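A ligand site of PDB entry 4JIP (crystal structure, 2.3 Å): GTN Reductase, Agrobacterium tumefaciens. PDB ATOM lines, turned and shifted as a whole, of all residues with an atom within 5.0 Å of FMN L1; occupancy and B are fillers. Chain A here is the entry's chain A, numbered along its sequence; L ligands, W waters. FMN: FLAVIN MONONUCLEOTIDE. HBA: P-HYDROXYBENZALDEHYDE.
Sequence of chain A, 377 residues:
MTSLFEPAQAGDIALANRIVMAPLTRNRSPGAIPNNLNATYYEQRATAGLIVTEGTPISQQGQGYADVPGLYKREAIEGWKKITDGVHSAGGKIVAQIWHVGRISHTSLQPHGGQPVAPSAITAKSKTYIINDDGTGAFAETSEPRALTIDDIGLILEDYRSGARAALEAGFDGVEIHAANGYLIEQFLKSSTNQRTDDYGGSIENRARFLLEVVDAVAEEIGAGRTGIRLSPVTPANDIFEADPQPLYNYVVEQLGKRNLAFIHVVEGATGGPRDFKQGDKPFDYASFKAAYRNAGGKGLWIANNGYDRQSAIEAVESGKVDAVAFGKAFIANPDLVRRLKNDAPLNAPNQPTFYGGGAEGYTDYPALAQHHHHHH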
ATOM      1  N   ALA A  22       5.236   1.000 -26.430  1.00  0.00           N
ATOM      2  CA  ALA A  22       6.278   1.132 -27.436  1.00  0.00           C
ATOM      3  C   ALA A  22       7.278  -0.009 -27.305  1.00  0.00           C
ATOM      4  O   ALA A  22       7.439  -0.577 -26.220  1.00  0.00           O
ATOM      5  CB  ALA A  22       6.975   2.481 -27.306  1.00  0.00           C
ATOM      6  N   PRO A  23       7.953  -0.365 -28.419  1.00  0.00           N
ATOM      7  CA  PRO A  23       9.057  -1.341 -28.368  1.00  0.00           C
ATOM      8  C   PRO A  23      10.222  -0.820 -27.536  1.00  0.00           C
ATOM      9  O   PRO A  23      10.662   0.314 -27.742  1.00  0.00           O
ATOM     10  CB  PRO A  23       9.487  -1.472 -29.842  1.00  0.00           C
ATOM     11  CG  PRO A  23       8.991  -0.204 -30.506  1.00  0.00           C
ATOM     12  CD  PRO A  23       7.709   0.129 -29.795  1.00  0.00           C
ATOM     13  N   LEU A  24      10.711  -1.639 -26.611  1.00  0.00           N
ATOM     14  CA  LEU A  24      11.777  -1.216 -25.703  1.00  0.00           C
ATOM     15  C   LEU A  24      12.843  -2.297 -25.460  1.00  0.00           C
ATOM     16  O   LEU A  24      12.650  -3.203 -24.650  1.00  0.00           O
ATOM     17  CB  LEU A  24      11.186  -0.751 -24.367  1.00  0.00           C
ATOM     18  CG  LEU A  24      10.200   0.422 -24.382  1.00  0.00           C
ATOM     19  CD1 LEU A  24       9.273   0.332 -23.181  1.00  0.00           C
ATOM     20  CD2 LEU A  24      10.914   1.772 -24.413  1.00  0.00           C
ATOM     21  N   THR A  25      13.949  -2.182 -26.185  1.00  0.00           N
ATOM     22  CA  THR A  25      15.157  -3.001 -25.980  1.00  0.00           C
ATOM     23  C   THR A  25      15.607  -2.918 -24.520  1.00  0.00           C
ATOM     24  O   THR A  25      15.894  -1.838 -24.021  1.00  0.00           O
ATOM     25  CB  THR A  25      16.314  -2.517 -26.899  1.00  0.00           C
ATOM     26  OG1 THR A  25      15.939  -2.674 -28.268  1.00  0.00           O
ATOM     27  CG2 THR A  25      17.596  -3.285 -26.627  1.00  0.00           C
ATOM     28  N   ARG A  26      15.654  -4.079 -23.842  1.00  0.00           N
ATOM     29  CA  ARG A  26      15.992  -4.150 -22.414  1.00  0.00           C
ATOM     30  C   ARG A  26      17.244  -5.019 -22.147  1.00  0.00           C
ATOM     31  O   ARG A  26      17.768  -5.043 -21.020  1.00  0.00           O
ATOM     32  CB  ARG A  26      14.812  -4.685 -21.597  1.00  0.00           C
ATOM     33  CG  ARG A  26      13.486  -3.961 -21.811  1.00  0.00           C
ATOM     34  CD  ARG A  26      13.629  -2.458 -21.632  1.00  0.00           C
ATOM     35  NE  ARG A  26      14.211  -2.130 -20.331  1.00  0.00           N
ATOM     36  CZ  ARG A  26      13.526  -2.022 -19.197  1.00  0.00           C
ATOM     37  NH1 ARG A  26      14.142  -1.731 -18.058  1.00  0.00           N
ATOM     38  NH2 ARG A  26      12.208  -2.206 -19.198  1.00  0.00           N
ATOM     39  N   GLU A  54      10.106  -5.475 -27.537  1.00  0.00           N
ATOM     40  CA  GLU A  54      11.442  -4.981 -27.827  1.00  0.00           C
ATOM     41  C   GLU A  54      11.843  -5.486 -29.222  1.00  0.00           C
ATOM     42  O   GLU A  54      11.271  -6.458 -29.714  1.00  0.00           O
ATOM     43  CB  GLU A  54      12.446  -5.542 -26.813  1.00  0.00           C
ATOM     44  CG  GLU A  54      12.596  -7.071 -26.849  1.00  0.00           C
ATOM     45  CD  GLU A  54      12.955  -7.652 -25.469  1.00  0.00           C
ATOM     46  OE1 GLU A  54      14.141  -7.621 -25.094  1.00  0.00           O
ATOM     47  OE2 GLU A  54      12.047  -8.134 -24.755  1.00  0.00           O
ATOM     48  N   GLY A  55      12.821  -4.826 -29.824  1.00  0.00           N
ATOM     49  CA  GLY A  55      13.342  -5.290 -31.100  1.00  0.00           C
ATOM     50  C   GLY A  55      13.762  -6.749 -30.990  1.00  0.00           C
ATOM     51  O   GLY A  55      14.507  -7.126 -30.084  1.00  0.00           O
ATOM     52  N   GLN A  97       8.232  -6.928 -32.788  1.00  0.00           N
ATOM     53  CA  GLN A  97       8.932  -5.985 -33.660  1.00  0.00           C
ATOM     54  C   GLN A  97      10.115  -6.685 -34.331  1.00  0.00           C
ATOM     55  O   GLN A  97      11.229  -6.698 -33.786  1.00  0.00           O
ATOM     56  CB  GLN A  97       9.404  -4.728 -32.911  1.00  0.00           C
ATOM     57  CG  GLN A  97       9.996  -3.671 -33.856  1.00  0.00           C
ATOM     58  CD  GLN A  97      10.646  -2.482 -33.160  1.00  0.00           C
ATOM     59  OE1 GLN A  97      11.410  -2.637 -32.210  1.00  0.00           O
ATOM     60  NE2 GLN A  97      10.351  -1.273 -33.653  1.00  0.00           N
ATOM     61  N   TRP A  99      13.250  -7.337 -36.444  1.00  0.00           N
ATOM     62  CA  TRP A  99      14.324  -6.366 -36.475  1.00  0.00           C
ATOM     63  C   TRP A  99      15.515  -6.821 -37.336  1.00  0.00           C
ATOM     64  O   TRP A  99      15.851  -8.000 -37.389  1.00  0.00           O
ATOM     65  CB  TRP A  99      14.799  -6.163 -35.028  1.00  0.00           C
ATOM     66  CG  TRP A  99      15.545  -4.906 -34.766  1.00  0.00           C
ATOM     67  CD1 TRP A  99      15.689  -3.836 -35.598  1.00  0.00           C
ATOM     68  CD2 TRP A  99      16.265  -4.579 -33.562  1.00  0.00           C
ATOM     69  NE1 TRP A  99      16.440  -2.868 -34.996  1.00  0.00           N
ATOM     70  CE2 TRP A  99      16.814  -3.295 -33.748  1.00  0.00           C
ATOM     71  CE3 TRP A  99      16.485  -5.245 -32.354  1.00  0.00           C
ATOM     72  CZ2 TRP A  99      17.575  -2.659 -32.758  1.00  0.00           C
ATOM     73  CZ3 TRP A  99      17.243  -4.612 -31.377  1.00  0.00           C
ATOM     74  CH2 TRP A  99      17.780  -3.327 -31.591  1.00  0.00           C
ATOM     75  N   HIS A 178      10.262  -3.269 -38.040  1.00  0.00           N
ATOM     76  CA  HIS A 178      11.109  -2.162 -37.606  1.00  0.00           C
ATOM     77  C   HIS A 178      11.807  -1.527 -38.818  1.00  0.00           C
ATOM     78  O   HIS A 178      12.768  -2.075 -39.366  1.00  0.00           O
ATOM     79  CB  HIS A 178      12.147  -2.630 -36.564  1.00  0.00           C
ATOM     80  CG  HIS A 178      12.798  -1.514 -35.820  1.00  0.00           C
ATOM     81  ND1 HIS A 178      12.760  -0.199 -36.240  1.00  0.00           N
ATOM     82  CD2 HIS A 178      13.506  -1.505 -34.660  1.00  0.00           C
ATOM     83  CE1 HIS A 178      13.413   0.560 -35.377  1.00  0.00           C
ATOM     84  NE2 HIS A 178      13.874  -0.202 -34.415  1.00  0.00           N
ATOM     85  N   ASN A 181      14.529   4.438 -36.830  1.00  0.00           N
ATOM     86  CA  ASN A 181      15.673   4.639 -35.958  1.00  0.00           C
ATOM     87  C   ASN A 181      17.056   4.256 -36.537  1.00  0.00           C
ATOM     88  O   ASN A 181      17.925   3.758 -35.823  1.00  0.00           O
ATOM     89  CB  ASN A 181      15.427   3.949 -34.609  1.00  0.00           C
ATOM     90  CG  ASN A 181      14.186   4.491 -33.916  1.00  0.00           C
ATOM     91  OD1 ASN A 181      13.802   5.652 -34.122  1.00  0.00           O
ATOM     92  ND2 ASN A 181      13.559   3.666 -33.082  1.00  0.00           N
ATOM     93  N   ARG A 230       7.020   0.315 -38.315  1.00  0.00           N
ATOM     94  CA  ARG A 230       7.373   1.551 -37.624  1.00  0.00           C
ATOM     95  C   ARG A 230       8.259   2.423 -38.513  1.00  0.00           C
ATOM     96  O   ARG A 230       9.219   1.949 -39.086  1.00  0.00           O
ATOM     97  CB  ARG A 230       8.096   1.250 -36.314  1.00  0.00           C
ATOM     98  CG  ARG A 230       8.305   2.487 -35.450  1.00  0.00           C
ATOM     99  CD  ARG A 230       8.818   2.143 -34.052  1.00  0.00           C
ATOM    100  NE  ARG A 230       8.133   2.931 -33.030  1.00  0.00           N
ATOM    101  CZ  ARG A 230       8.693   3.331 -31.898  1.00  0.00           C
ATOM    102  NH1 ARG A 230       9.949   3.014 -31.630  1.00  0.00           N
ATOM    103  NH2 ARG A 230       8.002   4.040 -31.012  1.00  0.00           N
ATOM    104  N   VAL A 267       7.284   7.509 -35.294  1.00  0.00           N
ATOM    105  CA  VAL A 267       8.042   8.257 -34.310  1.00  0.00           C
ATOM    106  C   VAL A 267       8.081   9.705 -34.774  1.00  0.00           C
ATOM    107  O   VAL A 267       8.621   9.998 -35.842  1.00  0.00           O
ATOM    108  CB  VAL A 267       9.484   7.733 -34.150  1.00  0.00           C
ATOM    109  CG1 VAL A 267      10.280   8.635 -33.220  1.00  0.00           C
ATOM    110  CG2 VAL A 267       9.476   6.316 -33.597  1.00  0.00           C
ATOM    111  N   THR A 271      13.948  10.516 -32.025  1.00  0.00           N
ATOM    112  CA  THR A 271      13.560   9.410 -31.151  1.00  0.00           C
ATOM    113  C   THR A 271      14.051   9.649 -29.732  1.00  0.00           C
ATOM    114  O   THR A 271      15.252   9.670 -29.477  1.00  0.00           O
ATOM    115  CB  THR A 271      14.097   8.048 -31.659  1.00  0.00           C
ATOM    116  OG1 THR A 271      13.850   7.924 -33.065  1.00  0.00           O
ATOM    117  CG2 THR A 271      13.429   6.892 -30.896  1.00  0.00           C
ATOM    118  N   GLY A 272      13.111   9.873 -28.801  1.00  0.00           N
ATOM    119  CA  GLY A 272      13.457  10.210 -27.442  1.00  0.00           C
ATOM    120  C   GLY A 272      13.942  11.648 -27.301  1.00  0.00           C
ATOM    121  O   GLY A 272      14.401  12.053 -26.223  1.00  0.00           O
ATOM    122  N   ASN A 305       4.004   8.196 -31.710  1.00  0.00           N
ATOM    123  CA  ASN A 305       4.932   8.107 -30.582  1.00  0.00           C
ATOM    124  C   ASN A 305       5.891   9.288 -30.505  1.00  0.00           C
ATOM    125  O   ASN A 305       6.170   9.927 -31.528  1.00  0.00           O
ATOM    126  CB  ASN A 305       5.729   6.791 -30.652  1.00  0.00           C
ATOM    127  CG  ASN A 305       6.933   6.791 -29.706  1.00  0.00           C
ATOM    128  OD1 ASN A 305       8.018   7.222 -30.065  1.00  0.00           O
ATOM    129  ND2 ASN A 305       6.717   6.332 -28.474  1.00  0.00           N
ATOM    130  N   ASN A 306       6.316   9.577 -29.270  1.00  0.00           N
ATOM    131  CA  ASN A 306       7.491  10.376 -28.900  1.00  0.00           C
ATOM    132  C   ASN A 306       7.174  11.630 -28.078  1.00  0.00           C
ATOM    133  O   ASN A 306       6.610  12.587 -28.596  1.00  0.00           O
ATOM    134  CB  ASN A 306       8.413  10.718 -30.081  1.00  0.00           C
ATOM    135  CG  ASN A 306       9.737  11.284 -29.640  1.00  0.00           C
ATOM    136  OD1 ASN A 306      10.402  10.727 -28.760  1.00  0.00           O
ATOM    137  ND2 ASN A 306      10.114  12.403 -30.224  1.00  0.00           N
ATOM    138  N   GLY A 307       7.548  11.600 -26.803  1.00  0.00           N
ATOM    139  CA  GLY A 307       7.335  12.736 -25.923  1.00  0.00           C
ATOM    140  C   GLY A 307       5.893  13.006 -25.556  1.00  0.00           C
ATOM    141  O   GLY A 307       5.567  14.098 -25.094  1.00  0.00           O
ATOM    142  N   TYR A 308       5.017  12.022 -25.745  1.00  0.00           N
ATOM    143  CA  TYR A 308       3.618  12.187 -25.354  1.00  0.00           C
ATOM    144  C   TYR A 308       3.422  12.019 -23.857  1.00  0.00           C
ATOM    145  O   TYR A 308       4.083  11.171 -23.246  1.00  0.00           O
ATOM    146  CB  TYR A 308       2.751  11.156 -26.079  1.00  0.00           C
ATOM    147  CG  TYR A 308       2.368  11.552 -27.473  1.00  0.00           C
ATOM    148  CD1 TYR A 308       1.333  12.441 -27.697  1.00  0.00           C
ATOM    149  CD2 TYR A 308       3.018  11.011 -28.580  1.00  0.00           C
ATOM    150  CE1 TYR A 308       0.966  12.809 -28.969  1.00  0.00           C
ATOM    151  CE2 TYR A 308       2.653  11.377 -29.874  1.00  0.00           C
ATOM    152  CZ  TYR A 308       1.626  12.276 -30.057  1.00  0.00           C
ATOM    153  OH  TYR A 308       1.249  12.635 -31.325  1.00  0.00           O
ATOM    154  N   ALA A 326       1.659   5.492 -28.583  1.00  0.00           N
ATOM    155  CA  ALA A 326       2.630   4.553 -28.019  1.00  0.00           C
ATOM    156  C   ALA A 326       3.534   5.253 -26.996  1.00  0.00           C
ATOM    157  O   ALA A 326       4.149   6.274 -27.301  1.00  0.00           O
ATOM    158  CB  ALA A 326       3.461   3.912 -29.118  1.00  0.00           C
ATOM    159  N   PHE A 327       3.604   4.685 -25.793  1.00  0.00           N
ATOM    160  CA  PHE A 327       4.492   5.196 -24.748  1.00  0.00           C
ATOM    161  C   PHE A 327       5.675   4.256 -24.529  1.00  0.00           C
ATOM    162  O   PHE A 327       5.505   3.039 -24.363  1.00  0.00           O
ATOM    163  CB  PHE A 327       3.739   5.368 -23.413  1.00  0.00           C
ATOM    164  CG  PHE A 327       2.507   6.239 -23.514  1.00  0.00           C
ATOM    165  CD1 PHE A 327       1.306   5.719 -23.957  1.00  0.00           C
ATOM    166  CD2 PHE A 327       2.555   7.580 -23.139  1.00  0.00           C
ATOM    167  CE1 PHE A 327       0.184   6.524 -24.050  1.00  0.00           C
ATOM    168  CE2 PHE A 327       1.433   8.385 -23.233  1.00  0.00           C
ATOM    169  CZ  PHE A 327       0.242   7.860 -23.684  1.00  0.00           C
ATOM    170  N   GLY A 328       6.873   4.816 -24.536  1.00  0.00           N
ATOM    171  CA  GLY A 328       8.071   4.060 -24.241  1.00  0.00           C
ATOM    172  C   GLY A 328       8.397   4.112 -22.752  1.00  0.00           C
ATOM    173  O   GLY A 328       7.958   3.251 -21.981  1.00  0.00           O
ATOM    174  N   LYS A 329       9.138   5.144 -22.373  1.00  0.00           N
ATOM    175  CA  LYS A 329       9.671   5.259 -21.014  1.00  0.00           C
ATOM    176  C   LYS A 329       8.618   5.163 -19.925  1.00  0.00           C
ATOM    177  O   LYS A 329       8.889   4.656 -18.843  1.00  0.00           O
ATOM    178  CB  LYS A 329      10.509   6.529 -20.866  1.00  0.00           C
ATOM    179  CG  LYS A 329      11.753   6.549 -21.747  1.00  0.00           C
ATOM    180  CD  LYS A 329      12.683   7.724 -21.438  1.00  0.00           C
ATOM    181  CE  LYS A 329      11.996   9.053 -21.665  1.00  0.00           C
ATOM    182  NZ  LYS A 329      11.543   9.227 -23.070  1.00  0.00           N
ATOM    183  N   ALA A 330       7.409   5.644 -20.208  1.00  0.00           N
ATOM    184  CA  ALA A 330       6.324   5.617 -19.227  1.00  0.00           C
ATOM    185  C   ALA A 330       5.892   4.177 -18.931  1.00  0.00           C
ATOM    186  O   ALA A 330       5.424   3.880 -17.833  1.00  0.00           O
ATOM    187  CB  ALA A 330       5.141   6.434 -19.713  1.00  0.00           C
ATOM    188  N   ILE A 332       8.005   1.530 -19.288  1.00  0.00           N
ATOM    189  CA  ILE A 332       9.099   0.998 -18.496  1.00  0.00           C
ATOM    190  C   ILE A 332       8.757   1.198 -17.022  1.00  0.00           C
ATOM    191  O   ILE A 332       8.773   0.264 -16.231  1.00  0.00           O
ATOM    192  CB  ILE A 332      10.446   1.703 -18.805  1.00  0.00           C
ATOM    193  CG1 ILE A 332      10.927   1.362 -20.222  1.00  0.00           C
ATOM    194  CG2 ILE A 332      11.493   1.331 -17.767  1.00  0.00           C
ATOM    195  CD1 ILE A 332      12.331   1.857 -20.528  1.00  0.00           C
ATOM    196  N   PHE A 355      17.722   0.741 -17.731  1.00  0.00           N
ATOM    197  CA  PHE A 355      17.052   0.475 -18.998  1.00  0.00           C
ATOM    198  C   PHE A 355      17.622  -0.797 -19.648  1.00  0.00           C
ATOM    199  O   PHE A 355      16.864  -1.669 -20.094  1.00  0.00           O
ATOM    200  CB  PHE A 355      17.205   1.656 -19.965  1.00  0.00           C
ATOM    201  CG  PHE A 355      16.293   2.822 -19.659  1.00  0.00           C
ATOM    202  CD1 PHE A 355      15.406   2.767 -18.589  1.00  0.00           C
ATOM    203  CD2 PHE A 355      16.313   3.963 -20.459  1.00  0.00           C
ATOM    204  CE1 PHE A 355      14.566   3.835 -18.311  1.00  0.00           C
ATOM    205  CE2 PHE A 355      15.476   5.033 -20.191  1.00  0.00           C
ATOM    206  CZ  PHE A 355      14.603   4.976 -19.115  1.00  0.00           C
ATOM    207  N   TYR A 356      18.940  -0.895 -19.665  1.00  0.00           N
ATOM    208  CA  TYR A 356      19.624  -1.944 -20.420  1.00  0.00           C
ATOM    209  C   TYR A 356      20.358  -2.958 -19.552  1.00  0.00           C
ATOM    210  O   TYR A 356      21.120  -2.583 -18.653  1.00  0.00           O
ATOM    211  CB  TYR A 356      20.630  -1.289 -21.370  1.00  0.00           C
ATOM    212  CG  TYR A 356      20.045  -0.138 -22.149  1.00  0.00           C
ATOM    213  CD1 TYR A 356      19.158  -0.354 -23.194  1.00  0.00           C
ATOM    214  CD2 TYR A 356      20.370   1.175 -21.830  1.00  0.00           C
ATOM    215  CE1 TYR A 356      18.631   0.693 -23.908  1.00  0.00           C
ATOM    216  CE2 TYR A 356      19.831   2.238 -22.544  1.00  0.00           C
ATOM    217  CZ  TYR A 356      18.958   1.983 -23.583  1.00  0.00           C
ATOM    218  OH  TYR A 356      18.417   3.019 -24.305  1.00  0.00           O
HETATM  219  N1  FMN L   1      12.350   1.761 -30.374  1.00  0.00           N
HETATM  220  C2  FMN L   1      12.254   0.700 -31.256  1.00  0.00           C
HETATM  221  O2  FMN L   1      11.695   0.827 -32.350  1.00  0.00           O
HETATM  222  N3  FMN L   1      12.824  -0.510 -30.937  1.00  0.00           N
HETATM  223  C4  FMN L   1      13.432  -0.678 -29.710  1.00  0.00           C
HETATM  224  O4  FMN L   1      13.927  -1.770 -29.426  1.00  0.00           O
HETATM  225  C4A FMN L   1      13.556   0.392 -28.836  1.00  0.00           C
HETATM  226  N5  FMN L   1      14.227   0.259 -27.639  1.00  0.00           N
HETATM  227  C5A FMN L   1      14.236   1.280 -26.705  1.00  0.00           C
HETATM  228  C6  FMN L   1      14.759   1.061 -25.439  1.00  0.00           C
HETATM  229  C7  FMN L   1      14.736   2.071 -24.487  1.00  0.00           C
HETATM  230  C7M FMN L   1      15.337   1.832 -23.136  1.00  0.00           C
HETATM  231  C8  FMN L   1      14.167   3.308 -24.798  1.00  0.00           C
HETATM  232  C8M FMN L   1      14.157   4.410 -23.783  1.00  0.00           C
HETATM  233  C9  FMN L   1      13.633   3.519 -26.061  1.00  0.00           C
HETATM  234  C9A FMN L   1      13.653   2.505 -27.026  1.00  0.00           C
HETATM  235  N10 FMN L   1      13.070   2.678 -28.274  1.00  0.00           N
HETATM  236  C10 FMN L   1      12.980   1.609 -29.156  1.00  0.00           C
HETATM  237  C1' FMN L   1      12.358   3.953 -28.616  1.00  0.00           C
HETATM  238  C2' FMN L   1      10.956   4.018 -28.004  1.00  0.00           C
HETATM  239  O2' FMN L   1      10.123   3.039 -28.578  1.00  0.00           O
HETATM  240  C3' FMN L   1      10.327   5.396 -28.181  1.00  0.00           C
HETATM  241  O3' FMN L   1      10.418   5.746 -29.552  1.00  0.00           O
HETATM  242  C4' FMN L   1      11.027   6.458 -27.330  1.00  0.00           C
HETATM  243  O4' FMN L   1      11.195   5.937 -26.027  1.00  0.00           O
HETATM  244  C5' FMN L   1      10.229   7.760 -27.264  1.00  0.00           C
HETATM  245  O5' FMN L   1       9.003   7.466 -26.661  1.00  0.00           O
HETATM  246  P   FMN L   1       8.609   8.007 -25.186  1.00  0.00           P
HETATM  247  O1P FMN L   1       7.191   7.573 -24.938  1.00  0.00           O
HETATM  248  O2P FMN L   1       9.538   7.388 -24.164  1.00  0.00           O
HETATM  249  O3P FMN L   1       8.727   9.505 -25.143  1.00  0.00           O
HETATM  250  C1' HBA L   2      17.692   1.895 -27.717  1.00  0.00           C
HETATM  251  O1' HBA L   2      18.335   1.004 -27.159  1.00  0.00           O
HETATM  252  C1  HBA L   2      16.964   1.659 -29.002  1.00  0.00           C
HETATM  253  C2  HBA L   2      17.002   0.440 -29.666  1.00  0.00           C
HETATM  254  C3  HBA L   2      16.309   0.276 -30.849  1.00  0.00           C
HETATM  255  C4  HBA L   2      15.562   1.305 -31.382  1.00  0.00           C
HETATM  256  C5  HBA L   2      15.528   2.526 -30.727  1.00  0.00           C
HETATM  257  C6  HBA L   2      16.211   2.696 -29.535  1.00  0.00           C
HETATM  258  O4  HBA L   2      14.879   1.149 -32.570  1.00  0.00           O
HETATM  259  O   HOH W   1       5.329   8.663 -26.699  1.00  0.00           O
HETATM  260  O   HOH W   2       6.567   7.622 -22.370  1.00  0.00           O
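OD1 of Asn 305 lies close to NH2 of Arg 230 (3.3 Å).
ND2 of Asn 305 lies within hydrogen-bond range of O of Ala 326, at 2.8 Å.
OD1 of Asn 306 lies within hydrogen-bond range of N of Gly 272 (2.8 Å).
N of Ala 22 is in hydrogen-bond range of O of Phe 327 (2.9 Å).
The side-chain amide oxygen (OD1) of Asn 181 sits at hydrogen-bond distance from the side-chain hydroxyl (OG1) of Thr 271, at 2.5 Å.
The backbone carbonyl oxygen (O) of Phe 355 sits at hydrogen-bond distance from the guanidinium group (NE) of Arg 26.
Water W2 bridges O1P of FMN L1 and N of Ala 330.
Water W1 lies within hydrogen-bond range of the backbone carbonyl oxygen (O) of Ala 326 (2.7 Å), an oxygen (O1P) of FMN L1 (2.8 Å), the backbone NH (N) of Asn 306 (2.9 Å) and the side-chain amide nitrogen (ND2) of Asn 305 (3.2 Å).
O4 of HBA L2 lies close to N3 of FMN L1 (3.1 Å).
N of Thr 25 sits at hydrogen-bond distance from N5 of FMN L1, at 2.9 Å.
OG1 of Thr 25 sits at hydrogen-bond distance from O4 of FMN L1.
An oxygen (O1P) of FMN L1 is in hydrogen-bond range of the backbone NH (N) of Gly 328.
NE2 of Gln 97 is in hydrogen-bond range of O2 of FMN L1 (2.8 Å).
The side-chain amide oxygen (OD1) of Asn 305 is in hydrogen-bond range of an oxygen (O3') of FMN L1, 2.9 Å away.
The guanidinium group (NH1) of Arg 230 sits at hydrogen-bond distance from an oxygen (O2) of FMN L1 (2.9 Å).
N of Lys 329 is in hydrogen-bond range of O2P of FMN L1, 2.9 Å away.
NZ of Lys 329 is in salt-bridge range of O2P of FMN L1 (2.9 Å).
The backbone carbonyl oxygen of Pro 23 sits at hydrogen-bond distance from an oxygen (O2') of FMN L1.
The backbone NH (N) of Gly 307 sits at hydrogen-bond distance from an oxygen (O3P) of FMN L1, at 2.9 Å.
A ring nitrogen (NE2) of His 178 sits at hydrogen-bond distance from an oxygen (O2) of FMN L1 (3.2 Å).
An oxygen (O4) of FMN L1 sits at hydrogen-bond distance from the backbone NH of Gly 55 (3.3 Å).
O2 of FMN L1 sits at hydrogen-bond distance from ND2 of Asn 181, 3.5 Å away.
NE2 of His 178 lies within hydrogen-bond range of O4 of HBA L2 (2.5 Å).
ND2 of Asn 181 is in hydrogen-bond range of O4 of HBA L2, at 2.9 Å.
OH of Tyr 356 lies close to O1' of HBA L2 (3.5 Å).
Merely in contact with FMN L1: Asn 306, Ala 22, Leu 24, Thr 271, Tyr 356, Phe 355, Phe 327, Gly 272 and Ile 332.
20 residues have an atom within 4 Å of FMN L1: Ala 22, Pro 23, Leu 24, Thr 25, Gly 55, Gln 97, His 178, Asn 181, Arg 230, Thr 271, Gly 272, Asn 305, Asn 306, Gly 307, Phe 327, Gly 328, Lys 329, Ile 332, Phe 355 and Tyr 356.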
